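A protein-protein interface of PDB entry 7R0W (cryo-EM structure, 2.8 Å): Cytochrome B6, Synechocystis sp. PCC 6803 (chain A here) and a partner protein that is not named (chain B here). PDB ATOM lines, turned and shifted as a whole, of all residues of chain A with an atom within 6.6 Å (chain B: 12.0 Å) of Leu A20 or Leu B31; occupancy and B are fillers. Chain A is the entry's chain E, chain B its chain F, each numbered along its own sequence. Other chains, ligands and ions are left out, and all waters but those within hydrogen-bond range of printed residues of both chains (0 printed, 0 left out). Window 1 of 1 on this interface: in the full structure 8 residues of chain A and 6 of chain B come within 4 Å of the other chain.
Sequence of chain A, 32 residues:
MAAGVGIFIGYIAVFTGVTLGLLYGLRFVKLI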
ATOM      1  N   PHE A  15     -24.886 -35.315   3.194  1.00  0.00           N
ATOM      2  CA  PHE A  15     -24.181 -34.519   4.187  1.00  0.00           C
ATOM      3  C   PHE A  15     -24.717 -33.094   4.278  1.00  0.00           C
ATOM      4  O   PHE A  15     -24.817 -32.552   5.380  1.00  0.00           O
ATOM      5  CB  PHE A  15     -22.687 -34.555   3.915  1.00  0.00           C
ATOM      6  CG  PHE A  15     -22.000 -35.682   4.621  1.00  0.00           C
ATOM      7  CD1 PHE A  15     -21.641 -35.561   5.951  1.00  0.00           C
ATOM      8  CD2 PHE A  15     -21.754 -36.878   3.972  1.00  0.00           C
ATOM      9  CE1 PHE A  15     -21.023 -36.601   6.612  1.00  0.00           C
ATOM     10  CE2 PHE A  15     -21.136 -37.921   4.628  1.00  0.00           C
ATOM     11  CZ  PHE A  15     -20.773 -37.784   5.951  1.00  0.00           C
ATOM     12  N   THR A  16     -25.019 -32.436   3.151  1.00  0.00           N
ATOM     13  CA  THR A  16     -25.621 -31.112   3.261  1.00  0.00           C
ATOM     14  C   THR A  16     -26.987 -31.175   3.931  1.00  0.00           C
ATOM     15  O   THR A  16     -27.358 -30.256   4.673  1.00  0.00           O
ATOM     16  CB  THR A  16     -25.732 -30.460   1.881  1.00  0.00           C
ATOM     17  OG1 THR A  16     -25.731 -29.034   2.024  1.00  0.00           O
ATOM     18  CG2 THR A  16     -27.008 -30.890   1.173  1.00  0.00           C
ATOM     19  N   GLY A  17     -27.718 -32.277   3.749  1.00  0.00           N
ATOM     20  CA  GLY A  17     -28.971 -32.435   4.461  1.00  0.00           C
ATOM     21  C   GLY A  17     -28.747 -32.588   5.947  1.00  0.00           C
ATOM     22  O   GLY A  17     -29.477 -32.013   6.753  1.00  0.00           O
ATOM     23  N   VAL A  18     -27.695 -33.309   6.328  1.00  0.00           N
ATOM     24  CA  VAL A  18     -27.399 -33.481   7.745  1.00  0.00           C
ATOM     25  C   VAL A  18     -26.947 -32.158   8.336  1.00  0.00           C
ATOM     26  O   VAL A  18     -27.313 -31.808   9.460  1.00  0.00           O
ATOM     27  CB  VAL A  18     -26.343 -34.583   7.944  1.00  0.00           C
ATOM     28  CG1 VAL A  18     -25.684 -34.458   9.315  1.00  0.00           C
ATOM     29  CG2 VAL A  18     -26.973 -35.954   7.779  1.00  0.00           C
ATOM     30  N   THR A  19     -26.185 -31.384   7.570  1.00  0.00           N
ATOM     31  CA  THR A  19     -25.650 -30.129   8.078  1.00  0.00           C
ATOM     32  C   THR A  19     -26.770 -29.127   8.303  1.00  0.00           C
ATOM     33  O   THR A  19     -26.861 -28.512   9.373  1.00  0.00           O
ATOM     34  CB  THR A  19     -24.613 -29.567   7.106  1.00  0.00           C
ATOM     35  OG1 THR A  19     -23.625 -30.566   6.823  1.00  0.00           O
ATOM     36  CG2 THR A  19     -23.934 -28.339   7.690  1.00  0.00           C
ATOM     37  N   LEU A  20     -27.665 -28.979   7.323  1.00  0.00           N
ATOM     38  CA  LEU A  20     -28.746 -28.017   7.493  1.00  0.00           C
ATOM     39  C   LEU A  20     -29.805 -28.526   8.461  1.00  0.00           C
ATOM     40  O   LEU A  20     -30.367 -27.734   9.228  1.00  0.00           O
ATOM     41  CB  LEU A  20     -29.379 -27.710   6.137  1.00  0.00           C
ATOM     42  CG  LEU A  20     -28.442 -27.234   5.022  1.00  0.00           C
ATOM     43  CD1 LEU A  20     -29.228 -26.490   3.963  1.00  0.00           C
ATOM     44  CD2 LEU A  20     -27.309 -26.361   5.548  1.00  0.00           C
ATOM     45  N   GLY A  21     -30.040 -29.840   8.501  1.00  0.00           N
ATOM     46  CA  GLY A  21     -30.915 -30.390   9.518  1.00  0.00           C
ATOM     47  C   GLY A  21     -30.404 -30.105  10.911  1.00  0.00           C
ATOM     48  O   GLY A  21     -31.142 -29.623  11.769  1.00  0.00           O
ATOM     49  N   LEU A  22     -29.112 -30.344  11.137  1.00  0.00           N
ATOM     50  CA  LEU A  22     -28.555 -30.137  12.464  1.00  0.00           C
ATOM     51  C   LEU A  22     -28.561 -28.661  12.811  1.00  0.00           C
ATOM     52  O   LEU A  22     -28.915 -28.286  13.931  1.00  0.00           O
ATOM     53  CB  LEU A  22     -27.135 -30.697  12.534  1.00  0.00           C
ATOM     54  CG  LEU A  22     -26.791 -31.640  13.687  1.00  0.00           C
ATOM     55  CD1 LEU A  22     -27.715 -32.848  13.724  1.00  0.00           C
ATOM     56  CD2 LEU A  22     -25.344 -32.083  13.584  1.00  0.00           C
ATOM     57  N   LEU A  23     -28.211 -27.803  11.856  1.00  0.00           N
ATOM     58  CA  LEU A  23     -28.118 -26.383  12.163  1.00  0.00           C
ATOM     59  C   LEU A  23     -29.492 -25.821  12.504  1.00  0.00           C
ATOM     60  O   LEU A  23     -29.670 -25.189  13.553  1.00  0.00           O
ATOM     61  CB  LEU A  23     -27.500 -25.636  10.982  1.00  0.00           C
ATOM     62  CG  LEU A  23     -27.385 -24.119  11.115  1.00  0.00           C
ATOM     63  CD1 LEU A  23     -26.169 -23.742  11.943  1.00  0.00           C
ATOM     64  CD2 LEU A  23     -27.311 -23.483   9.747  1.00  0.00           C
ATOM     65  N   TYR A  24     -30.491 -26.078  11.654  1.00  0.00           N
ATOM     66  CA  TYR A  24     -31.816 -25.529  11.914  1.00  0.00           C
ATOM     67  C   TYR A  24     -32.477 -26.197  13.112  1.00  0.00           C
ATOM     68  O   TYR A  24     -33.213 -25.536  13.854  1.00  0.00           O
ATOM     69  CB  TYR A  24     -32.687 -25.671  10.669  1.00  0.00           C
ATOM     70  CG  TYR A  24     -32.451 -24.576   9.656  1.00  0.00           C
ATOM     71  CD1 TYR A  24     -31.460 -24.698   8.695  1.00  0.00           C
ATOM     72  CD2 TYR A  24     -33.214 -23.419   9.665  1.00  0.00           C
ATOM     73  CE1 TYR A  24     -31.237 -23.700   7.769  1.00  0.00           C
ATOM     74  CE2 TYR A  24     -32.998 -22.415   8.744  1.00  0.00           C
ATOM     75  CZ  TYR A  24     -32.008 -22.561   7.798  1.00  0.00           C
ATOM     76  OH  TYR A  24     -31.789 -21.563   6.878  1.00  0.00           O
ATOM     77  N   GLY A  25     -32.208 -27.482  13.348  1.00  0.00           N
ATOM     78  CA  GLY A  25     -32.797 -28.147  14.495  1.00  0.00           C
ATOM     79  C   GLY A  25     -32.217 -27.629  15.794  1.00  0.00           C
ATOM     80  O   GLY A  25     -32.946 -27.350  16.749  1.00  0.00           O
ATOM     81  N   ARG A  27     -30.752 -24.734  16.244  1.00  0.00           N
ATOM     82  CA  ARG A  27     -31.225 -23.370  16.423  1.00  0.00           C
ATOM     83  C   ARG A  27     -32.664 -23.358  16.915  1.00  0.00           C
ATOM     84  O   ARG A  27     -33.054 -22.468  17.679  1.00  0.00           O
ATOM     85  CB  ARG A  27     -31.110 -22.597  15.110  1.00  0.00           C
ATOM     86  CG  ARG A  27     -29.744 -21.986  14.869  1.00  0.00           C
ATOM     87  CD  ARG A  27     -29.594 -21.522  13.433  1.00  0.00           C
ATOM     88  NE  ARG A  27     -28.343 -20.807  13.218  1.00  0.00           N
ATOM     89  CZ  ARG A  27     -28.046 -20.128  12.119  1.00  0.00           C
ATOM     90  NH1 ARG A  27     -28.894 -20.048  11.106  1.00  0.00           N
ATOM     91  NH2 ARG A  27     -26.870 -19.513  12.034  1.00  0.00           N
ATOM     92  N   LEU B  20     -15.470 -26.739  -6.535  1.00  0.00           N
ATOM     93  CA  LEU B  20     -16.781 -27.166  -6.076  1.00  0.00           C
ATOM     94  C   LEU B  20     -16.869 -27.097  -4.559  1.00  0.00           C
ATOM     95  O   LEU B  20     -17.939 -26.814  -4.022  1.00  0.00           O
ATOM     96  CB  LEU B  20     -17.084 -28.572  -6.597  1.00  0.00           C
ATOM     97  CG  LEU B  20     -18.468 -29.176  -6.322  1.00  0.00           C
ATOM     98  CD1 LEU B  20     -18.505 -29.920  -5.012  1.00  0.00           C
ATOM     99  CD2 LEU B  20     -19.565 -28.114  -6.369  1.00  0.00           C
ATOM    100  N   GLY B  21     -15.764 -27.330  -3.849  1.00  0.00           N
ATOM    101  CA  GLY B  21     -15.790 -27.165  -2.407  1.00  0.00           C
ATOM    102  C   GLY B  21     -16.008 -25.713  -2.033  1.00  0.00           C
ATOM    103  O   GLY B  21     -16.844 -25.394  -1.181  1.00  0.00           O
ATOM    104  N   LEU B  22     -15.242 -24.812  -2.655  1.00  0.00           N
ATOM    105  CA  LEU B  22     -15.470 -23.389  -2.425  1.00  0.00           C
ATOM    106  C   LEU B  22     -16.929 -23.034  -2.685  1.00  0.00           C
ATOM    107  O   LEU B  22     -17.590 -22.384  -1.860  1.00  0.00           O
ATOM    108  CB  LEU B  22     -14.561 -22.548  -3.320  1.00  0.00           C
ATOM    109  CG  LEU B  22     -13.233 -22.063  -2.739  1.00  0.00           C
ATOM    110  CD1 LEU B  22     -12.505 -23.160  -1.977  1.00  0.00           C
ATOM    111  CD2 LEU B  22     -12.368 -21.500  -3.844  1.00  0.00           C
ATOM    112  N   ALA B  23     -17.454 -23.476  -3.830  1.00  0.00           N
ATOM    113  CA  ALA B  23     -18.809 -23.101  -4.204  1.00  0.00           C
ATOM    114  C   ALA B  23     -19.811 -23.665  -3.214  1.00  0.00           C
ATOM    115  O   ALA B  23     -20.752 -22.976  -2.813  1.00  0.00           O
ATOM    116  CB  ALA B  23     -19.117 -23.587  -5.619  1.00  0.00           C
ATOM    117  N   TRP B  24     -19.630 -24.920  -2.805  1.00  0.00           N
ATOM    118  CA  TRP B  24     -20.620 -25.557  -1.957  1.00  0.00           C
ATOM    119  C   TRP B  24     -20.563 -25.009  -0.544  1.00  0.00           C
ATOM    120  O   TRP B  24     -21.582 -25.009   0.150  1.00  0.00           O
ATOM    121  CB  TRP B  24     -20.425 -27.069  -1.945  1.00  0.00           C
ATOM    122  CG  TRP B  24     -21.581 -27.777  -1.341  1.00  0.00           C
ATOM    123  CD1 TRP B  24     -21.636 -28.357  -0.113  1.00  0.00           C
ATOM    124  CD2 TRP B  24     -22.879 -27.936  -1.919  1.00  0.00           C
ATOM    125  NE1 TRP B  24     -22.880 -28.894   0.102  1.00  0.00           N
ATOM    126  CE2 TRP B  24     -23.663 -28.648  -0.993  1.00  0.00           C
ATOM    127  CE3 TRP B  24     -23.449 -27.557  -3.137  1.00  0.00           C
ATOM    128  CZ2 TRP B  24     -24.988 -28.987  -1.245  1.00  0.00           C
ATOM    129  CZ3 TRP B  24     -24.764 -27.894  -3.385  1.00  0.00           C
ATOM    130  CH2 TRP B  24     -25.519 -28.602  -2.445  1.00  0.00           C
ATOM    131  N   GLY B  25     -19.422 -24.459  -0.128  1.00  0.00           N
ATOM    132  CA  GLY B  25     -19.376 -23.856   1.187  1.00  0.00           C
ATOM    133  C   GLY B  25     -19.924 -22.449   1.173  1.00  0.00           C
ATOM    134  O   GLY B  25     -20.515 -22.005   2.162  1.00  0.00           O
ATOM    135  N   PHE B  26     -19.839 -21.766   0.029  1.00  0.00           N
ATOM    136  CA  PHE B  26     -20.577 -20.513  -0.095  1.00  0.00           C
ATOM    137  C   PHE B  26     -22.074 -20.784  -0.174  1.00  0.00           C
ATOM    138  O   PHE B  26     -22.887 -20.014   0.357  1.00  0.00           O
ATOM    139  CB  PHE B  26     -20.097 -19.746  -1.323  1.00  0.00           C
ATOM    140  CG  PHE B  26     -18.890 -18.899  -1.065  1.00  0.00           C
ATOM    141  CD1 PHE B  26     -18.960 -17.808  -0.218  1.00  0.00           C
ATOM    142  CD2 PHE B  26     -17.681 -19.195  -1.666  1.00  0.00           C
ATOM    143  CE1 PHE B  26     -17.850 -17.028   0.022  1.00  0.00           C
ATOM    144  CE2 PHE B  26     -16.567 -18.420  -1.429  1.00  0.00           C
ATOM    145  CZ  PHE B  26     -16.651 -17.337  -0.582  1.00  0.00           C
ATOM    146  N   VAL B  27     -22.443 -21.919  -0.767  1.00  0.00           N
ATOM    147  CA  VAL B  27     -23.840 -22.325  -0.802  1.00  0.00           C
ATOM    148  C   VAL B  27     -24.328 -22.595   0.610  1.00  0.00           C
ATOM    149  O   VAL B  27     -25.434 -22.201   0.984  1.00  0.00           O
ATOM    150  CB  VAL B  27     -24.017 -23.554  -1.711  1.00  0.00           C
ATOM    151  CG1 VAL B  27     -25.351 -24.233  -1.439  1.00  0.00           C
ATOM    152  CG2 VAL B  27     -23.912 -23.150  -3.169  1.00  0.00           C
ATOM    153  N   ILE B  28     -23.512 -23.272   1.417  1.00  0.00           N
ATOM    154  CA  ILE B  28     -23.921 -23.570   2.783  1.00  0.00           C
ATOM    155  C   ILE B  28     -24.010 -22.284   3.592  1.00  0.00           C
ATOM    156  O   ILE B  28     -24.890 -22.137   4.449  1.00  0.00           O
ATOM    157  CB  ILE B  28     -22.962 -24.579   3.437  1.00  0.00           C
ATOM    158  CG1 ILE B  28     -23.064 -25.942   2.753  1.00  0.00           C
ATOM    159  CG2 ILE B  28     -23.275 -24.727   4.913  1.00  0.00           C
ATOM    160  CD1 ILE B  28     -21.817 -26.778   2.896  1.00  0.00           C
ATOM    161  N   ILE B  29     -23.107 -21.334   3.341  1.00  0.00           N
ATOM    162  CA  ILE B  29     -23.220 -20.036   3.999  1.00  0.00           C
ATOM    163  C   ILE B  29     -24.575 -19.412   3.688  1.00  0.00           C
ATOM    164  O   ILE B  29     -25.260 -18.903   4.581  1.00  0.00           O
ATOM    165  CB  ILE B  29     -22.061 -19.118   3.574  1.00  0.00           C
ATOM    166  CG1 ILE B  29     -20.748 -19.608   4.186  1.00  0.00           C
ATOM    167  CG2 ILE B  29     -22.328 -17.687   4.000  1.00  0.00           C
ATOM    168  CD1 ILE B  29     -19.518 -19.164   3.431  1.00  0.00           C
ATOM    169  N   LYS B  30     -24.980 -19.433   2.417  1.00  0.00           N
ATOM    170  CA  LYS B  30     -26.252 -18.806   2.060  1.00  0.00           C
ATOM    171  C   LYS B  30     -27.441 -19.598   2.602  1.00  0.00           C
ATOM    172  O   LYS B  30     -28.392 -19.013   3.127  1.00  0.00           O
ATOM    173  CB  LYS B  30     -26.349 -18.608   0.542  1.00  0.00           C
ATOM    174  CG  LYS B  30     -27.636 -17.898   0.005  1.00  0.00           C
ATOM    175  CD  LYS B  30     -28.436 -17.115   1.055  1.00  0.00           C
ATOM    176  CE  LYS B  30     -29.664 -16.414   0.522  1.00  0.00           C
ATOM    177  NZ  LYS B  30     -30.233 -15.534   1.587  1.00  0.00           N
ATOM    178  N   LEU B  31     -27.349 -20.922   2.640  1.00  0.00           N
ATOM    179  CA  LEU B  31     -28.528 -21.680   3.030  1.00  0.00           C
ATOM    180  C   LEU B  31     -28.845 -21.501   4.505  1.00  0.00           C
ATOM    181  O   LEU B  31     -29.961 -21.816   4.929  1.00  0.00           O
ATOM    182  CB  LEU B  31     -28.345 -23.157   2.680  1.00  0.00           C
ATOM    183  CG  LEU B  31     -28.289 -23.460   1.173  1.00  0.00           C
ATOM    184  CD1 LEU B  31     -28.274 -24.956   0.909  1.00  0.00           C
ATOM    185  CD2 LEU B  31     -29.397 -22.778   0.368  1.00  0.00           C
ATOM    186  N   GLN B  32     -27.897 -21.007   5.292  1.00  0.00           N
ATOM    187  CA  GLN B  32     -28.172 -20.713   6.685  1.00  0.00           C
ATOM    188  C   GLN B  32     -28.827 -19.337   6.780  1.00  0.00           C
ATOM    189  O   GLN B  32     -28.672 -18.486   5.899  1.00  0.00           O
ATOM    190  CB  GLN B  32     -26.887 -20.748   7.509  1.00  0.00           C
ATOM    191  CG  GLN B  32     -26.164 -19.415   7.583  1.00  0.00           C
ATOM    192  CD  GLN B  32     -24.731 -19.557   8.034  1.00  0.00           C
ATOM    193  OE1 GLN B  32     -24.433 -20.303   8.965  1.00  0.00           O
ATOM    194  NE2 GLN B  32     -23.825 -18.901   7.323  1.00  0.00           N
ATOM    195  N   GLY B  33     -29.570 -19.118   7.862  1.00  0.00           N
ATOM    196  CA  GLY B  33     -30.283 -17.867   8.064  1.00  0.00           C
ATOM    197  C   GLY B  33     -29.512 -16.928   8.972  1.00  0.00           C
ATOM    198  O   GLY B  33     -29.138 -17.291  10.090  1.00  0.00           O
ATOM    199  N   SER B  34     -29.281 -15.717   8.477  1.00  0.00           N
ATOM    200  CA  SER B  34     -28.540 -14.707   9.224  1.00  0.00           C
ATOM    201  C   SER B  34     -29.493 -13.822  10.019  1.00  0.00           C
ATOM    202  O   SER B  34     -30.512 -14.290  10.526  1.00  0.00           O
ATOM    203  CB  SER B  34     -27.692 -13.852   8.281  1.00  0.00           C
ATOM    204  OG  SER B  34     -28.366 -13.617   7.057  1.00  0.00           O
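The side-chain hydroxyl (OH) of Tyr A24 lies within hydrogen-bond range of the backbone NH (N) of Gly B33 (3.4 Å).
OH of Tyr A24 is in hydrogen-bond range of O of Leu B31.
The guanidinium group (NH1) of Arg A27 sits at hydrogen-bond distance from the backbone carbonyl oxygen (O) of Gly B33, 2.9 Å away.
The indole nitrogen of Trp B24 sits close to the side-chain hydroxyl of Thr A16 (3.4 Å).
The backbone carbonyl oxygen of Ile B29 lies within hydrogen-bond range of the side-chain amide nitrogen of Gln B32, 3.1 Å away.
Among the printed residues, merely in contact across the chains: Leu A20 with Leu B31 (3.5 Å), Leu A23 with Gln B32 (3.6 Å), Tyr A24 with Gln B32 (3.7 Å) and Arg A27 with Gln B32 (3.998 Å).
Thr A16 touches one residue of chain B.
No residue of chain B comes within 4 Å of Val A18.
Leu A20 touches just one residue of chain B: Leu B31 (3.5 Å).
No residue of chain B comes within 4 Å of Gly A21.
Gly A25 touches none of the printed residues of chain B.
Of the printed residues of chain B, Arg A27 touches Gln B32 (3.998 Å) and Gly B33 (2.9 Å).
Of the printed residues of chain A, Trp B24 touches Thr A16.
Of chain A, only Leu A20 and Tyr A24 come within 4 Å of Leu B31.
Printed residues of chain A within 4 Å of Gln B32: Leu A23, Tyr A24 and Arg A27.
Printed residues of chain A within 4 Å of Gly B33: Tyr A24 (3.4 Å) and Arg A27 (2.9 Å).
The nearest residue of chain B that does not touch Leu A20 is Ile B28 (4.4 Å).
Of the 12 printed residues of chain A, 5 touch a printed residue of chain B.
Printed residues of chain A that touch a printed residue of chain B: Thr A16, Leu A20, Leu A23, Tyr A24 and Arg A27.
Among the printed residues, no Asp or Glu carboxylate lies within 4 Å of a Lys or Arg side-chain nitrogen of the other chain.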
